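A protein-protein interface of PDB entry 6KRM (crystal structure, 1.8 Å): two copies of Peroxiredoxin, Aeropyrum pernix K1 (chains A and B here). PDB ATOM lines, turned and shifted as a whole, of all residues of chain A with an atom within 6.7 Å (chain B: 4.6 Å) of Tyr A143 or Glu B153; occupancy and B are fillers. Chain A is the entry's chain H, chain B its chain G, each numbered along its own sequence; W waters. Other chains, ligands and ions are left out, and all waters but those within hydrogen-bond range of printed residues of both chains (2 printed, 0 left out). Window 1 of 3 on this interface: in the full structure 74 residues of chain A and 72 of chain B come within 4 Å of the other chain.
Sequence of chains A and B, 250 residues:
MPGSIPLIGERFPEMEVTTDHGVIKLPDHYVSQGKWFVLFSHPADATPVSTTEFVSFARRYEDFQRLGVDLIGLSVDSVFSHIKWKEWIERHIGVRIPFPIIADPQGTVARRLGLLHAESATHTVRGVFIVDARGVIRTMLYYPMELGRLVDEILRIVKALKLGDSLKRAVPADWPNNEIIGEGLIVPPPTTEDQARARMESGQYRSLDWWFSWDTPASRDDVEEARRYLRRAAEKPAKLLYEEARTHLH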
ATOM      1  N   GLU A  53     -17.420   9.371   4.228  1.00  0.00           N
ATOM      2  CA  GLU A  53     -18.647   9.815   4.942  1.00  0.00           C
ATOM      3  C   GLU A  53     -19.575  10.505   3.967  1.00  0.00           C
ATOM      4  O   GLU A  53     -20.805  10.273   4.074  1.00  0.00           O
ATOM      5  CB  GLU A  53     -18.358  10.732   6.107  1.00  0.00           C
ATOM      6  CG  GLU A  53     -17.541  10.030   7.166  1.00  0.00           C
ATOM      7  CD  GLU A  53     -17.237  10.930   8.337  1.00  0.00           C
ATOM      8  OE1 GLU A  53     -16.687  12.014   8.071  1.00  0.00           O
ATOM      9  OE2 GLU A  53     -17.505  10.522   9.527  1.00  0.00           O
ATOM     10  N   HIS A 117     -11.999  21.109  18.590  1.00  0.00           N
ATOM     11  CA  HIS A 117     -11.562  20.355  19.783  1.00  0.00           C
ATOM     12  C   HIS A 117     -10.022  20.330  19.837  1.00  0.00           C
ATOM     13  O   HIS A 117      -9.372  21.065  19.099  1.00  0.00           O
ATOM     14  CB  HIS A 117     -12.234  18.978  19.793  1.00  0.00           C
ATOM     15  CG  HIS A 117     -13.706  19.030  19.966  1.00  0.00           C
ATOM     16  ND1 HIS A 117     -14.378  18.077  20.701  1.00  0.00           N
ATOM     17  CD2 HIS A 117     -14.618  19.946  19.596  1.00  0.00           C
ATOM     18  CE1 HIS A 117     -15.661  18.374  20.703  1.00  0.00           C
ATOM     19  NE2 HIS A 117     -15.841  19.526  20.055  1.00  0.00           N
ATOM     20  N   GLU A 119      -7.770  17.935  19.110  1.00  0.00           N
ATOM     21  CA  GLU A 119      -7.052  17.140  18.097  1.00  0.00           C
ATOM     22  C   GLU A 119      -6.536  18.059  16.995  1.00  0.00           C
ATOM     23  O   GLU A 119      -5.597  17.665  16.293  1.00  0.00           O
ATOM     24  CB  GLU A 119      -7.961  16.107  17.435  1.00  0.00           C
ATOM     25  CG  GLU A 119      -8.090  14.808  18.188  1.00  0.00           C
ATOM     26  CD  GLU A 119      -8.700  13.733  17.291  1.00  0.00           C
ATOM     27  OE1 GLU A 119      -8.048  12.685  17.125  1.00  0.00           O
ATOM     28  OE2 GLU A 119      -9.800  13.975  16.688  1.00  0.00           O
ATOM     29  N   THR A 124     -12.394  21.344  12.005  1.00  0.00           N
ATOM     30  CA  THR A 124     -13.467  20.868  12.884  1.00  0.00           C
ATOM     31  C   THR A 124     -13.326  19.367  13.094  1.00  0.00           C
ATOM     32  O   THR A 124     -12.875  18.646  12.177  1.00  0.00           O
ATOM     33  CB  THR A 124     -14.860  21.176  12.326  1.00  0.00           C
ATOM     34  OG1 THR A 124     -15.035  20.492  11.091  1.00  0.00           O
ATOM     35  CG2 THR A 124     -15.068  22.660  12.103  1.00  0.00           C
ATOM     36  N   VAL A 125     -13.751  18.891  14.263  1.00  0.00           N
ATOM     37  CA  VAL A 125     -14.014  17.450  14.435  1.00  0.00           C
ATOM     38  C   VAL A 125     -15.222  17.037  13.563  1.00  0.00           C
ATOM     39  O   VAL A 125     -15.784  17.819  12.784  1.00  0.00           O
ATOM     40  CB  VAL A 125     -14.230  17.130  15.930  1.00  0.00           C
ATOM     41  CG1 VAL A 125     -12.937  17.371  16.713  1.00  0.00           C
ATOM     42  CG2 VAL A 125     -15.413  17.874  16.502  1.00  0.00           C
ATOM     43  N   ARG A 126     -15.661  15.803  13.788  1.00  0.00           N
ATOM     44  CA  ARG A 126     -16.760  15.193  13.030  1.00  0.00           C
ATOM     45  C   ARG A 126     -17.980  15.336  13.900  1.00  0.00           C
ATOM     46  O   ARG A 126     -18.404  14.305  14.494  1.00  0.00           O
ATOM     47  CB  ARG A 126     -16.424  13.743  12.687  1.00  0.00           C
ATOM     48  CG  ARG A 126     -15.210  13.572  11.786  1.00  0.00           C
ATOM     49  CD  ARG A 126     -15.050  12.147  11.247  1.00  0.00           C
ATOM     50  NE  ARG A 126     -13.685  12.023  10.779  1.00  0.00           N
ATOM     51  CZ  ARG A 126     -13.286  12.460   9.570  1.00  0.00           C
ATOM     52  NH1 ARG A 126     -12.012  12.502   9.287  1.00  0.00           N
ATOM     53  NH2 ARG A 126     -14.156  12.887   8.671  1.00  0.00           N
ATOM     54  N   GLY A 127     -18.539  16.546  13.930  1.00  0.00           N
ATOM     55  CA  GLY A 127     -19.718  16.873  14.731  1.00  0.00           C
ATOM     56  C   GLY A 127     -20.998  16.583  13.966  1.00  0.00           C
ATOM     57  O   GLY A 127     -20.985  16.541  12.719  1.00  0.00           O
ATOM     58  N   VAL A 128     -22.042  16.220  14.693  1.00  0.00           N
ATOM     59  CA  VAL A 128     -23.394  15.978  14.121  1.00  0.00           C
ATOM     60  C   VAL A 128     -24.394  16.693  15.027  1.00  0.00           C
ATOM     61  O   VAL A 128     -24.443  16.393  16.270  1.00  0.00           O
ATOM     62  CB  VAL A 128     -23.726  14.478  13.991  1.00  0.00           C
ATOM     63  CG1 VAL A 128     -25.076  14.227  13.324  1.00  0.00           C
ATOM     64  CG2 VAL A 128     -22.661  13.675  13.271  1.00  0.00           C
ATOM     65  N   LEU A 141     -23.536  14.418  18.261  1.00  0.00           N
ATOM     66  CA  LEU A 141     -22.456  13.404  18.260  1.00  0.00           C
ATOM     67  C   LEU A 141     -21.160  14.112  17.920  1.00  0.00           C
ATOM     68  O   LEU A 141     -21.150  14.996  17.009  1.00  0.00           O
ATOM     69  CB  LEU A 141     -22.756  12.319  17.222  1.00  0.00           C
ATOM     70  CG  LEU A 141     -24.199  11.809  17.166  1.00  0.00           C
ATOM     71  CD1 LEU A 141     -24.367  10.895  15.961  1.00  0.00           C
ATOM     72  CD2 LEU A 141     -24.575  11.069  18.460  1.00  0.00           C
ATOM     73  N   TYR A 142     -20.071  13.687  18.553  1.00  0.00           N
ATOM     74  CA  TYR A 142     -18.733  14.239  18.258  1.00  0.00           C
ATOM     75  C   TYR A 142     -17.775  13.067  18.071  1.00  0.00           C
ATOM     76  O   TYR A 142     -17.333  12.464  19.045  1.00  0.00           O
ATOM     77  CB  TYR A 142     -18.256  15.154  19.395  1.00  0.00           C
ATOM     78  CG  TYR A 142     -19.111  16.384  19.548  1.00  0.00           C
ATOM     79  CD1 TYR A 142     -18.853  17.553  18.832  1.00  0.00           C
ATOM     80  CD2 TYR A 142     -20.194  16.374  20.397  1.00  0.00           C
ATOM     81  CE1 TYR A 142     -19.666  18.667  18.957  1.00  0.00           C
ATOM     82  CE2 TYR A 142     -21.001  17.494  20.554  1.00  0.00           C
ATOM     83  CZ  TYR A 142     -20.720  18.644  19.848  1.00  0.00           C
ATOM     84  OH  TYR A 142     -21.564  19.712  19.958  1.00  0.00           O
ATOM     85  N   TYR A 143     -17.532  12.758  16.810  1.00  0.00           N
ATOM     86  CA  TYR A 143     -16.542  11.760  16.357  1.00  0.00           C
ATOM     87  C   TYR A 143     -15.234  12.482  16.075  1.00  0.00           C
ATOM     88  O   TYR A 143     -15.219  13.673  15.779  1.00  0.00           O
ATOM     89  CB  TYR A 143     -17.076  11.041  15.123  1.00  0.00           C
ATOM     90  CG  TYR A 143     -18.064   9.942  15.422  1.00  0.00           C
ATOM     91  CD1 TYR A 143     -19.327  10.239  15.908  1.00  0.00           C
ATOM     92  CD2 TYR A 143     -17.779   8.633  15.133  1.00  0.00           C
ATOM     93  CE1 TYR A 143     -20.259   9.250  16.179  1.00  0.00           C
ATOM     94  CE2 TYR A 143     -18.710   7.630  15.375  1.00  0.00           C
ATOM     95  CZ  TYR A 143     -19.964   7.941  15.872  1.00  0.00           C
ATOM     96  OH  TYR A 143     -20.884   6.949  16.092  1.00  0.00           O
ATOM     97  N   PRO A 144     -14.102  11.760  16.169  1.00  0.00           N
ATOM     98  CA  PRO A 144     -12.781  12.348  15.966  1.00  0.00           C
ATOM     99  C   PRO A 144     -12.277  12.283  14.513  1.00  0.00           C
ATOM    100  O   PRO A 144     -12.897  11.631  13.669  1.00  0.00           O
ATOM    101  CB  PRO A 144     -11.946  11.452  16.928  1.00  0.00           C
ATOM    102  CG  PRO A 144     -12.537  10.064  16.770  1.00  0.00           C
ATOM    103  CD  PRO A 144     -14.035  10.348  16.558  1.00  0.00           C
ATOM    104  N   MET A 145     -11.116  12.891  14.230  1.00  0.00           N
ATOM    105  CA  MET A 145     -10.520  12.885  12.871  1.00  0.00           C
ATOM    106  C   MET A 145     -10.311  11.448  12.378  1.00  0.00           C
ATOM    107  O   MET A 145     -10.503  11.183  11.181  1.00  0.00           O
ATOM    108  CB  MET A 145      -9.157  13.578  12.850  1.00  0.00           C
ATOM    109  CG  MET A 145      -9.152  14.964  13.413  1.00  0.00           C
ATOM    110  SD  MET A 145     -10.618  15.909  12.961  1.00  0.00           S
ATOM    111  CE  MET A 145     -10.053  17.540  13.459  1.00  0.00           C
ATOM    112  N   GLU A 146      -9.941  10.545  13.259  1.00  0.00           N
ATOM    113  CA  GLU A 146      -9.399   9.215  12.845  1.00  0.00           C
ATOM    114  C   GLU A 146     -10.523   8.186  12.628  1.00  0.00           C
ATOM    115  O   GLU A 146     -10.208   7.013  12.258  1.00  0.00           O
ATOM    116  CB  GLU A 146      -8.388   8.675  13.857  1.00  0.00           C
ATOM    117  CG  GLU A 146      -8.924   8.439  15.223  1.00  0.00           C
ATOM    118  CD  GLU A 146      -8.852   9.612  16.190  1.00  0.00           C
ATOM    119  OE1 GLU A 146      -8.882   9.321  17.409  1.00  0.00           O
ATOM    120  OE2 GLU A 146      -8.734  10.826  15.729  1.00  0.00           O
ATOM    121  N   LEU A 147     -11.783   8.553  12.863  1.00  0.00           N
ATOM    122  CA  LEU A 147     -12.875   7.526  12.885  1.00  0.00           C
ATOM    123  C   LEU A 147     -14.090   8.060  12.138  1.00  0.00           C
ATOM    124  O   LEU A 147     -14.692   9.018  12.674  1.00  0.00           O
ATOM    125  CB  LEU A 147     -13.289   7.347  14.335  1.00  0.00           C
ATOM    126  CG  LEU A 147     -13.822   6.015  14.843  1.00  0.00           C
ATOM    127  CD1 LEU A 147     -14.930   6.198  15.859  1.00  0.00           C
ATOM    128  CD2 LEU A 147     -14.064   4.925  13.823  1.00  0.00           C
ATOM    129  N   GLY A 148     -14.490   7.414  11.066  1.00  0.00           N
ATOM    130  CA  GLY A 148     -15.707   7.765  10.316  1.00  0.00           C
ATOM    131  C   GLY A 148     -16.966   7.398  11.085  1.00  0.00           C
ATOM    132  O   GLY A 148     -16.958   6.441  11.901  1.00  0.00           O
ATOM    133  N   ARG A 149     -18.034   8.129  10.828  1.00  0.00           N
ATOM    134  CA  ARG A 149     -19.325   7.898  11.499  1.00  0.00           C
ATOM    135  C   ARG A 149     -20.002   6.623  10.939  1.00  0.00           C
ATOM    136  O   ARG A 149     -19.571   6.047   9.895  1.00  0.00           O
ATOM    137  CB  ARG A 149     -20.162   9.170  11.368  1.00  0.00           C
ATOM    138  CG  ARG A 149     -19.718  10.264  12.319  1.00  0.00           C
ATOM    139  CD  ARG A 149     -20.126  11.667  11.915  1.00  0.00           C
ATOM    140  NE  ARG A 149     -19.308  12.159  10.844  1.00  0.00           N
ATOM    141  CZ  ARG A 149     -19.087  13.442  10.557  1.00  0.00           C
ATOM    142  NH1 ARG A 149     -19.691  14.409  11.229  1.00  0.00           N
ATOM    143  NH2 ARG A 149     -18.278  13.746   9.564  1.00  0.00           N
ATOM    144  N   LEU A 150     -20.980   6.138  11.704  1.00  0.00           N
ATOM    145  CA  LEU A 150     -21.906   5.063  11.291  1.00  0.00           C
ATOM    146  C   LEU A 150     -23.201   5.752  10.861  1.00  0.00           C
ATOM    147  O   LEU A 150     -23.996   6.153  11.725  1.00  0.00           O
ATOM    148  CB  LEU A 150     -22.144   4.099  12.463  1.00  0.00           C
ATOM    149  CG  LEU A 150     -22.949   2.864  12.070  1.00  0.00           C
ATOM    150  CD1 LEU A 150     -22.065   1.927  11.266  1.00  0.00           C
ATOM    151  CD2 LEU A 150     -23.526   2.154  13.280  1.00  0.00           C
ATOM    152  N   GLU A 153     -26.766   4.848  12.004  1.00  0.00           N
ATOM    153  CA  GLU A 153     -27.201   5.229  13.380  1.00  0.00           C
ATOM    154  C   GLU A 153     -27.838   6.611  13.348  1.00  0.00           C
ATOM    155  O   GLU A 153     -28.769   6.854  14.098  1.00  0.00           O
ATOM    156  CB  GLU A 153     -26.062   5.155  14.398  1.00  0.00           C
ATOM    157  CG  GLU A 153     -26.431   5.718  15.781  1.00  0.00           C
ATOM    158  CD  GLU A 153     -27.601   5.075  16.517  1.00  0.00           C
ATOM    159  OE1 GLU A 153     -28.204   4.151  15.925  1.00  0.00           O
ATOM    160  OE2 GLU A 153     -27.932   5.515  17.660  1.00  0.00           O
ATOM    161  N   ASP A 174     -31.401   0.367  21.676  1.00  0.00           N
ATOM    162  CA  ASP A 174     -31.163  -0.615  20.587  1.00  0.00           C
ATOM    163  C   ASP A 174     -32.479  -0.835  19.831  1.00  0.00           C
ATOM    164  O   ASP A 174     -32.524  -1.776  19.014  1.00  0.00           O
ATOM    165  CB  ASP A 174     -30.579  -1.925  21.115  1.00  0.00           C
ATOM    166  CG  ASP A 174     -29.397  -1.790  22.071  1.00  0.00           C
ATOM    167  OD1 ASP A 174     -28.506  -0.974  21.797  1.00  0.00           O
ATOM    168  OD2 ASP A 174     -29.429  -2.431  23.145  1.00  0.00           O
ATOM    169  N   ILE B   8     -12.703  16.490  22.644  1.00  0.00           N
ATOM    170  CA  ILE B   8     -11.933  15.374  22.042  1.00  0.00           C
ATOM    171  C   ILE B   8     -10.448  15.768  22.033  1.00  0.00           C
ATOM    172  O   ILE B   8     -10.129  16.893  21.591  1.00  0.00           O
ATOM    173  CB  ILE B   8     -12.471  15.033  20.640  1.00  0.00           C
ATOM    174  CG1 ILE B   8     -13.856  14.394  20.718  1.00  0.00           C
ATOM    175  CG2 ILE B   8     -11.488  14.129  19.940  1.00  0.00           C
ATOM    176  CD1 ILE B   8     -14.513  14.213  19.374  1.00  0.00           C
ATOM    177  N   THR B 139     -14.022  10.279  21.919  1.00  0.00           N
ATOM    178  CA  THR B 139     -15.346  10.453  21.268  1.00  0.00           C
ATOM    179  C   THR B 139     -16.313  10.895  22.341  1.00  0.00           C
ATOM    180  O   THR B 139     -16.223  10.349  23.462  1.00  0.00           O
ATOM    181  CB  THR B 139     -15.772   9.142  20.579  1.00  0.00           C
ATOM    182  OG1 THR B 139     -14.958   8.883  19.438  1.00  0.00           O
ATOM    183  CG2 THR B 139     -17.180   9.173  20.015  1.00  0.00           C
ATOM    184  N   LEU B 141     -20.731  11.455  22.798  1.00  0.00           N
ATOM    185  CA  LEU B 141     -22.098  11.380  22.224  1.00  0.00           C
ATOM    186  C   LEU B 141     -23.071  11.991  23.224  1.00  0.00           C
ATOM    187  O   LEU B 141     -22.921  11.740  24.438  1.00  0.00           O
ATOM    188  CB  LEU B 141     -22.461   9.925  21.993  1.00  0.00           C
ATOM    189  CG  LEU B 141     -21.421   9.071  21.283  1.00  0.00           C
ATOM    190  CD1 LEU B 141     -21.861   7.632  21.339  1.00  0.00           C
ATOM    191  CD2 LEU B 141     -21.234   9.537  19.853  1.00  0.00           C
ATOM    192  N   LEU B 150     -27.615   3.213  21.031  1.00  0.00           N
ATOM    193  CA  LEU B 150     -27.300   1.961  20.296  1.00  0.00           C
ATOM    194  C   LEU B 150     -25.970   1.490  20.831  1.00  0.00           C
ATOM    195  O   LEU B 150     -24.949   1.987  20.371  1.00  0.00           O
ATOM    196  CB  LEU B 150     -27.223   2.232  18.802  1.00  0.00           C
ATOM    197  CG  LEU B 150     -27.091   0.968  17.948  1.00  0.00           C
ATOM    198  CD1 LEU B 150     -28.409   0.211  17.937  1.00  0.00           C
ATOM    199  CD2 LEU B 150     -26.678   1.306  16.534  1.00  0.00           C
ATOM    200  N   VAL B 151     -25.980   0.588  21.810  1.00  0.00           N
ATOM    201  CA  VAL B 151     -24.740   0.252  22.559  1.00  0.00           C
ATOM    202  C   VAL B 151     -23.699  -0.425  21.648  1.00  0.00           C
ATOM    203  O   VAL B 151     -22.485  -0.283  21.945  1.00  0.00           O
ATOM    204  CB  VAL B 151     -25.078  -0.553  23.828  1.00  0.00           C
ATOM    205  CG1 VAL B 151     -23.841  -0.930  24.626  1.00  0.00           C
ATOM    206  CG2 VAL B 151     -26.021   0.254  24.707  1.00  0.00           C
ATOM    207  N   ASP B 152     -24.116  -1.162  20.612  1.00  0.00           N
ATOM    208  CA  ASP B 152     -23.164  -1.837  19.702  1.00  0.00           C
ATOM    209  C   ASP B 152     -22.290  -0.797  18.988  1.00  0.00           C
ATOM    210  O   ASP B 152     -21.180  -1.145  18.661  1.00  0.00           O
ATOM    211  CB  ASP B 152     -23.914  -2.780  18.747  1.00  0.00           C
ATOM    212  CG  ASP B 152     -24.436  -4.011  19.500  1.00  0.00           C
ATOM    213  OD1 ASP B 152     -23.666  -4.634  20.212  1.00  0.00           O
ATOM    214  OD2 ASP B 152     -25.608  -4.291  19.394  1.00  0.00           O
ATOM    215  N   GLU B 153     -22.784   0.410  18.730  1.00  0.00           N
ATOM    216  CA  GLU B 153     -21.989   1.487  18.081  1.00  0.00           C
ATOM    217  C   GLU B 153     -20.880   1.907  19.040  1.00  0.00           C
ATOM    218  O   GLU B 153     -19.786   2.185  18.562  1.00  0.00           O
ATOM    219  CB  GLU B 153     -22.852   2.668  17.677  1.00  0.00           C
ATOM    220  CG  GLU B 153     -22.054   3.841  17.104  1.00  0.00           C
ATOM    221  CD  GLU B 153     -21.099   3.540  15.957  1.00  0.00           C
ATOM    222  OE1 GLU B 153     -21.017   2.380  15.520  1.00  0.00           O
ATOM    223  OE2 GLU B 153     -20.473   4.484  15.458  1.00  0.00           O
ATOM    224  N   ILE B 154     -21.121   1.900  20.355  1.00  0.00           N
ATOM    225  CA  ILE B 154     -20.063   2.226  21.357  1.00  0.00           C
ATOM    226  C   ILE B 154     -18.965   1.171  21.295  1.00  0.00           C
ATOM    227  O   ILE B 154     -17.781   1.528  21.231  1.00  0.00           O
ATOM    228  CB  ILE B 154     -20.620   2.407  22.778  1.00  0.00           C
ATOM    229  CG1 ILE B 154     -21.676   3.506  22.821  1.00  0.00           C
ATOM    230  CG2 ILE B 154     -19.490   2.663  23.750  1.00  0.00           C
ATOM    231  CD1 ILE B 154     -22.339   3.669  24.172  1.00  0.00           C
ATOM    232  N   LEU B 155     -19.326  -0.108  21.218  1.00  0.00           N
ATOM    233  CA  LEU B 155     -18.314  -1.163  20.988  1.00  0.00           C
ATOM    234  C   LEU B 155     -17.565  -0.927  19.669  1.00  0.00           C
ATOM    235  O   LEU B 155     -16.348  -1.125  19.693  1.00  0.00           O
ATOM    236  CB  LEU B 155     -18.995  -2.528  20.976  1.00  0.00           C
ATOM    237  CG  LEU B 155     -19.436  -3.032  22.343  1.00  0.00           C
ATOM    238  CD1 LEU B 155     -20.363  -4.220  22.177  1.00  0.00           C
ATOM    239  CD2 LEU B 155     -18.238  -3.383  23.210  1.00  0.00           C
ATOM    240  N   ARG B 156     -18.259  -0.647  18.567  1.00  0.00           N
ATOM    241  CA  ARG B 156     -17.628  -0.480  17.236  1.00  0.00           C
ATOM    242  C   ARG B 156     -16.632   0.687  17.331  1.00  0.00           C
ATOM    243  O   ARG B 156     -15.511   0.545  16.808  1.00  0.00           O
ATOM    244  CB  ARG B 156     -18.665  -0.262  16.123  1.00  0.00           C
ATOM    245  CG  ARG B 156     -18.092  -0.278  14.703  1.00  0.00           C
ATOM    246  CD  ARG B 156     -19.004   0.324  13.642  1.00  0.00           C
ATOM    247  NE  ARG B 156     -19.059   1.786  13.753  1.00  0.00           N
ATOM    248  CZ  ARG B 156     -18.268   2.627  13.103  1.00  0.00           C
ATOM    249  NH1 ARG B 156     -17.357   2.183  12.251  1.00  0.00           N
ATOM    250  NH2 ARG B 156     -18.355   3.924  13.354  1.00  0.00           N
ATOM    251  N   ILE B 157     -16.988   1.775  18.008  1.00  0.00           N
ATOM    252  CA  ILE B 157     -16.068   2.961  18.134  1.00  0.00           C
ATOM    253  C   ILE B 157     -14.775   2.517  18.832  1.00  0.00           C
ATOM    254  O   ILE B 157     -13.683   2.871  18.358  1.00  0.00           O
ATOM    255  CB  ILE B 157     -16.777   4.092  18.899  1.00  0.00           C
ATOM    256  CG1 ILE B 157     -17.875   4.691  18.031  1.00  0.00           C
ATOM    257  CG2 ILE B 157     -15.810   5.146  19.394  1.00  0.00           C
ATOM    258  CD1 ILE B 157     -18.919   5.469  18.801  1.00  0.00           C
HETATM  259  O   HOH W   1     -15.809   4.217  11.091  1.00  0.00           O
HETATM  260  O   HOH W   2     -26.858  -1.888  19.806  1.00  0.00           O
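N of Val B151 sits at hydrogen-bond distance from OD1 of Asp A174 (3.0 Å). The backbone carbonyl oxygen (O) of Gly A148 is in hydrogen-bond range of the guanidinium group (NH2) of Arg B156, 3.2 Å away. The side-chain hydroxyl (OH) of Tyr A143 lies within hydrogen-bond range of the side-chain carboxylate (OE2) of Glu B153 (2.6 Å). ND1 of His A117 is in hydrogen-bond range of N of Ile B8, 3.0 Å away.
The side-chain carboxylate (OE2) of Glu A119 is in hydrogen-bond range of the backbone NH (N) of Met A145 (3.0 Å). The backbone carbonyl oxygen of Gly A127 is in hydrogen-bond range of the guanidinium group of Arg A149. N of Val A128 is in hydrogen-bond range of O of Leu A141, at 2.8 Å. OE1 of Glu B153 is in salt-bridge range of NE of Arg B156, 2.7 Å away. The side-chain carboxylate (OE2) of Glu A53 lies within salt-bridge range of the guanidinium group (NE) of Arg A149 (2.8 Å). The side-chain carboxylate (OE2) of Glu A146 lies close to the side-chain carboxylate (OE1) of Glu A119.
Ile B8 touches Tyr A142. O of Tyr A142 touches CG2 of Thr B139 (3.4 Å). Tyr A143 touches Ile B8. Tyr A143 touches Leu B141 (CE1 to CD2, 3.8 Å). CD of Pro A144 touches OG1 of Thr B139, 3.4 Å away. Ile B157 touches Leu A147. OE1 of Glu B153 touches CD2 of Leu A150, 3.4 Å away. Arg B156 touches Leu A150 (NH2 to N, 3.8 Å). Leu B150 touches Glu A153 (CD2 to OE1, 3.3 Å). CA of Leu B150 touches OD1 of Asp A174 (3.5 Å).
Of the printed residues of chain B, His A117 touches Ile B8 (3.0 Å). Of the printed residues of chain B, Glu A119 touches Ile B8 (3.6 Å). Gly A127 touches none of the printed residues of chain B. Of chain B, only Ile B8, Leu B141, Glu B153 and Ile B157 come within 4 Å of Tyr A143. Of the printed residues of chain B, Leu A150 touches Glu B153 and Arg B156. Printed residues of chain A within 4 Å of Glu B153: Tyr A143 (2.6 Å) and Leu A150 (3.4 Å). The nearest residue of chain B that does not touch Tyr A143 is Arg B156 (4.2 Å). The nearest residue of chain A that does not touch Glu B153 is Glu A153 (4.9 Å).
Hydrophobic or aromatic side chains of chain A that line the printed part of chain B: His A117, Leu A141, Tyr A142, Tyr A143, Pro A144, Leu A147 and Leu A150. Along chain A the printed residues that touch a printed residue of chain B span positions 117 to 174. Hydrophobic or aromatic side chains of chain B within 4 Å of the printed part of chain A: Ile B8, Leu B141, Leu B150 and Ile B157. Among the printed residues, 18 pairs touch across the chains. Among the printed residues, no Asp or Glu carboxylate lies within 4 Å of a Lys or Arg side-chain nitrogen of the other chain.
Leu B141 touches its own counterpart, Leu A141. Leu A150 touches Glu B153, and with the chains exchanged Glu A153 touches Leu B150. Positions printed for both chains: 141, 150 and 153. Of the 18 pairs that touch across the chains among the printed residues, 3 have their exchanged pair printed and touching as well.
Water W1 bridges O of Gly A148 (2.6 Å) and NH1 of Arg B156 (2.8 Å). Water W2 lies within hydrogen-bond range of OD2 of Asp B152, OD1 of Asp A174 and N of Val B151.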
